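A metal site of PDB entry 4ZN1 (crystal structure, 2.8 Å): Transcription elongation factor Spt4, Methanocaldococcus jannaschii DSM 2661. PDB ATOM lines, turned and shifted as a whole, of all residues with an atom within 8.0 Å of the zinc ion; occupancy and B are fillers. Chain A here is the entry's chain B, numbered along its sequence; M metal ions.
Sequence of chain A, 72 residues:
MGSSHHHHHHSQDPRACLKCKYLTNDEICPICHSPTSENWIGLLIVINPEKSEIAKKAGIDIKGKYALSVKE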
ATOM      1  N   ALA A  16       1.302  -9.119  21.460  1.00  0.00           N
ATOM      2  CA  ALA A  16       0.671  -9.202  22.766  1.00  0.00           C
ATOM      3  C   ALA A  16      -0.819  -8.863  22.665  1.00  0.00           C
ATOM      4  O   ALA A  16      -1.170  -7.821  22.094  1.00  0.00           O
ATOM      5  CB  ALA A  16       1.364  -8.241  23.714  1.00  0.00           C
ATOM      6  N   CYS A  17      -1.657  -9.754  23.217  1.00  0.00           N
ATOM      7  CA  CYS A  17      -3.121  -9.588  23.241  1.00  0.00           C
ATOM      8  C   CYS A  17      -3.514  -8.258  23.877  1.00  0.00           C
ATOM      9  O   CYS A  17      -2.978  -7.899  24.937  1.00  0.00           O
ATOM     10  CB  CYS A  17      -3.777 -10.704  24.045  1.00  0.00           C
ATOM     11  SG  CYS A  17      -5.563 -10.537  24.357  1.00  0.00           S
ATOM     12  N   LEU A  18      -4.433  -7.545  23.235  1.00  0.00           N
ATOM     13  CA  LEU A  18      -4.890  -6.251  23.754  1.00  0.00           C
ATOM     14  C   LEU A  18      -5.615  -6.414  25.102  1.00  0.00           C
ATOM     15  O   LEU A  18      -5.438  -5.583  26.017  1.00  0.00           O
ATOM     16  CB  LEU A  18      -5.780  -5.547  22.717  1.00  0.00           C
ATOM     17  N   LYS A  19      -6.381  -7.500  25.249  1.00  0.00           N
ATOM     18  CA  LYS A  19      -7.134  -7.786  26.476  1.00  0.00           C
ATOM     19  C   LYS A  19      -6.212  -8.261  27.601  1.00  0.00           C
ATOM     20  O   LYS A  19      -5.936  -7.495  28.524  1.00  0.00           O
ATOM     21  CB  LYS A  19      -8.235  -8.829  26.220  1.00  0.00           C
ATOM     22  N   CYS A  20      -5.733  -9.502  27.510  1.00  0.00           N
ATOM     23  CA  CYS A  20      -5.051 -10.182  28.638  1.00  0.00           C
ATOM     24  C   CYS A  20      -3.518 -10.074  28.679  1.00  0.00           C
ATOM     25  O   CYS A  20      -2.928 -10.517  29.658  1.00  0.00           O
ATOM     26  CB  CYS A  20      -5.438 -11.674  28.678  1.00  0.00           C
ATOM     27  SG  CYS A  20      -5.020 -12.628  27.196  1.00  0.00           S
ATOM     28  N   LYS A  21      -2.902  -9.499  27.652  1.00  0.00           N
ATOM     29  CA  LYS A  21      -1.432  -9.293  27.561  1.00  0.00           C
ATOM     30  C   LYS A  21      -0.610 -10.552  27.213  1.00  0.00           C
ATOM     31  O   LYS A  21       0.630 -10.490  27.197  1.00  0.00           O
ATOM     32  CB  LYS A  21      -0.865  -8.595  28.831  1.00  0.00           C
ATOM     33  CG  LYS A  21      -0.901  -7.073  28.783  1.00  0.00           C
ATOM     34  CD  LYS A  21      -0.562  -6.391  30.104  1.00  0.00           C
ATOM     35  CE  LYS A  21      -1.650  -6.493  31.153  1.00  0.00           C
ATOM     36  NZ  LYS A  21      -3.032  -6.205  30.657  1.00  0.00           N
ATOM     37  N   TYR A  22      -1.276 -11.663  26.895  1.00  0.00           N
ATOM     38  CA  TYR A  22      -0.631 -12.940  26.599  1.00  0.00           C
ATOM     39  C   TYR A  22       0.145 -12.831  25.301  1.00  0.00           C
ATOM     40  O   TYR A  22      -0.381 -12.325  24.308  1.00  0.00           O
ATOM     41  CB  TYR A  22      -1.664 -14.057  26.462  1.00  0.00           C
ATOM     42  CG  TYR A  22      -1.072 -15.428  26.241  1.00  0.00           C
ATOM     43  CD1 TYR A  22      -0.708 -16.240  27.314  1.00  0.00           C
ATOM     44  CD2 TYR A  22      -0.890 -15.922  24.941  1.00  0.00           C
ATOM     45  CE1 TYR A  22      -0.176 -17.506  27.106  1.00  0.00           C
ATOM     46  CE2 TYR A  22      -0.350 -17.183  24.731  1.00  0.00           C
ATOM     47  CZ  TYR A  22       0.006 -17.966  25.807  1.00  0.00           C
ATOM     48  OH  TYR A  22       0.529 -19.215  25.609  1.00  0.00           O
ATOM     49  N   LEU A  23       1.380 -13.335  25.300  1.00  0.00           N
ATOM     50  CA  LEU A  23       2.262 -13.221  24.150  1.00  0.00           C
ATOM     51  C   LEU A  23       2.102 -14.387  23.196  1.00  0.00           C
ATOM     52  O   LEU A  23       2.249 -15.558  23.565  1.00  0.00           O
ATOM     53  CB  LEU A  23       3.724 -13.137  24.574  1.00  0.00           C
ATOM     54  CG  LEU A  23       4.205 -11.906  25.332  1.00  0.00           C
ATOM     55  CD1 LEU A  23       5.722 -11.945  25.446  1.00  0.00           C
ATOM     56  CD2 LEU A  23       3.770 -10.627  24.639  1.00  0.00           C
ATOM     57  N   THR A  24       1.839 -14.038  21.933  1.00  0.00           N
ATOM     58  CA  THR A  24       1.661 -14.991  20.853  1.00  0.00           C
ATOM     59  C   THR A  24       2.075 -14.349  19.529  1.00  0.00           C
ATOM     60  O   THR A  24       2.233 -13.130  19.442  1.00  0.00           O
ATOM     61  CB  THR A  24       0.198 -15.456  20.764  1.00  0.00           C
ATOM     62  OG1 THR A  24       0.068 -16.441  19.743  1.00  0.00           O
ATOM     63  CG2 THR A  24      -0.737 -14.281  20.458  1.00  0.00           C
ATOM     64  N   ILE A  28      -4.895 -13.202  16.586  1.00  0.00           N
ATOM     65  CA  ILE A  28      -5.906 -13.340  17.643  1.00  0.00           C
ATOM     66  C   ILE A  28      -5.338 -14.186  18.794  1.00  0.00           C
ATOM     67  O   ILE A  28      -4.626 -15.171  18.550  1.00  0.00           O
ATOM     68  CB  ILE A  28      -7.208 -13.977  17.119  1.00  0.00           C
ATOM     69  N   CYS A  29      -5.650 -13.792  20.029  1.00  0.00           N
ATOM     70  CA  CYS A  29      -5.105 -14.449  21.229  1.00  0.00           C
ATOM     71  C   CYS A  29      -5.690 -15.857  21.434  1.00  0.00           C
ATOM     72  O   CYS A  29      -6.898 -16.048  21.298  1.00  0.00           O
ATOM     73  CB  CYS A  29      -5.333 -13.559  22.470  1.00  0.00           C
ATOM     74  SG  CYS A  29      -5.153 -14.342  24.095  1.00  0.00           S
ATOM     75  N   PRO A  30      -4.819 -16.853  21.748  1.00  0.00           N
ATOM     76  CA  PRO A  30      -5.342 -18.201  22.027  1.00  0.00           C
ATOM     77  C   PRO A  30      -6.253 -18.299  23.257  1.00  0.00           C
ATOM     78  O   PRO A  30      -7.177 -19.123  23.258  1.00  0.00           O
ATOM     79  CB  PRO A  30      -4.067 -19.037  22.251  1.00  0.00           C
ATOM     80  CG  PRO A  30      -2.986 -18.289  21.550  1.00  0.00           C
ATOM     81  CD  PRO A  30      -3.343 -16.852  21.749  1.00  0.00           C
ATOM     82  N   ILE A  31      -6.014 -17.472  24.266  1.00  0.00           N
ATOM     83  CA  ILE A  31      -6.713 -17.588  25.551  1.00  0.00           C
ATOM     84  C   ILE A  31      -8.161 -17.153  25.334  1.00  0.00           C
ATOM     85  O   ILE A  31      -9.094 -17.911  25.609  1.00  0.00           O
ATOM     86  CB  ILE A  31      -6.042 -16.760  26.697  1.00  0.00           C
ATOM     87  CG1 ILE A  31      -4.528 -17.000  26.774  1.00  0.00           C
ATOM     88  CG2 ILE A  31      -6.662 -17.105  28.049  1.00  0.00           C
ATOM     89  CD1 ILE A  31      -4.085 -18.459  26.662  1.00  0.00           C
ATOM     90  N   CYS A  32      -8.321 -15.937  24.831  1.00  0.00           N
ATOM     91  CA  CYS A  32      -9.601 -15.415  24.362  1.00  0.00           C
ATOM     92  C   CYS A  32      -9.253 -14.875  22.979  1.00  0.00           C
ATOM     93  O   CYS A  32      -8.180 -14.314  22.813  1.00  0.00           O
ATOM     94  CB  CYS A  32     -10.152 -14.355  25.326  1.00  0.00           C
ATOM     95  SG  CYS A  32      -8.950 -13.098  25.871  1.00  0.00           S
ATOM     96  N   HIS A  33     -10.130 -15.046  21.999  1.00  0.00           N
ATOM     97  CA  HIS A  33      -9.831 -14.610  20.624  1.00  0.00           C
ATOM     98  C   HIS A  33      -9.995 -13.080  20.588  1.00  0.00           C
ATOM     99  O   HIS A  33     -11.007 -12.574  20.100  1.00  0.00           O
ATOM    100  CB  HIS A  33     -10.736 -15.282  19.595  1.00  0.00           C
ATOM    101  N   SER A  34      -9.003 -12.375  21.120  1.00  0.00           N
ATOM    102  CA  SER A  34      -8.972 -10.915  21.170  1.00  0.00           C
ATOM    103  C   SER A  34      -7.772 -10.448  20.332  1.00  0.00           C
ATOM    104  O   SER A  34      -6.783 -11.175  20.196  1.00  0.00           O
ATOM    105  CB  SER A  34      -8.853 -10.413  22.605  1.00  0.00           C
ATOM    106  N   PRO A  35      -7.867  -9.241  19.754  1.00  0.00           N
ATOM    107  CA  PRO A  35      -6.805  -8.793  18.856  1.00  0.00           C
ATOM    108  C   PRO A  35      -5.495  -8.521  19.583  1.00  0.00           C
ATOM    109  O   PRO A  35      -5.505  -8.006  20.716  1.00  0.00           O
ATOM    110  CB  PRO A  35      -7.358  -7.497  18.245  1.00  0.00           C
ATOM    111  CG  PRO A  35      -8.806  -7.459  18.597  1.00  0.00           C
ATOM    112  CD  PRO A  35      -8.919  -8.219  19.881  1.00  0.00           C
ATOM    113  N   THR A  36      -4.389  -8.861  18.927  1.00  0.00           N
ATOM    114  CA  THR A  36      -3.064  -8.699  19.485  1.00  0.00           C
ATOM    115  C   THR A  36      -2.338  -7.625  18.691  1.00  0.00           C
ATOM    116  O   THR A  36      -2.552  -7.464  17.495  1.00  0.00           O
ATOM    117  CB  THR A  36      -2.268 -10.040  19.484  1.00  0.00           C
ATOM    118  OG1 THR A  36      -1.889 -10.386  18.145  1.00  0.00           O
ATOM    119  N   TYR A  66       3.868 -12.967  29.183  1.00  0.00           N
ATOM    120  CA  TYR A  66       2.913 -11.861  29.180  1.00  0.00           C
ATOM    121  C   TYR A  66       3.648 -10.538  29.036  1.00  0.00           C
ATOM    122  O   TYR A  66       4.684 -10.356  29.653  1.00  0.00           O
ATOM    123  CB  TYR A  66       2.135 -11.820  30.498  1.00  0.00           C
ATOM    124  CG  TYR A  66       1.119 -12.914  30.672  1.00  0.00           C
ATOM    125  CD1 TYR A  66      -0.148 -12.806  30.118  1.00  0.00           C
ATOM    126  CD2 TYR A  66       1.432 -14.065  31.394  1.00  0.00           C
ATOM    127  CE1 TYR A  66      -1.091 -13.814  30.277  1.00  0.00           C
ATOM    128  CE2 TYR A  66       0.492 -15.074  31.567  1.00  0.00           C
ATOM    129  CZ  TYR A  66      -0.764 -14.948  31.003  1.00  0.00           C
ATOM    130  OH  TYR A  66      -1.663 -15.958  31.187  1.00  0.00           O
HETATM  131 ZN    ZN M   1      -6.087 -12.416  25.433  1.00  0.00          ZN
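Of the 19 residues printed, 4 come within 4 Å of the zinc ion. The nearest printed residue that does not touch the zinc ion is Lys 19 (4.3 Å).
The zinc ion is bound by SG of Cys 20 (2.1 Å), SG of Cys 17 (2.2 Å) and SG of Cys 29 (2.5 Å). The zinc ion has three donor atoms within binding distance. Slightly farther from the zinc ion lies the side-chain sulfur (SG) of Cys 32 (3.0 Å).
The side-chain sulfur of Cys 29 lies close to the backbone carbonyl oxygen of Cys 32 (3.3 Å). N of Cys 17 is in hydrogen-bond range of O of Tyr 22 (3.1 Å). N of Cys 29 sits at hydrogen-bond distance from O of Ser 34, at 2.9 Å. The side-chain sulfur (SG) of Cys 17 sits close to the backbone NH (N) of Lys 19, at 3.3 Å. The backbone NH (N) of Ile 31 lies close to the side-chain sulfur (SG) of Cys 29 (3.3 Å).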
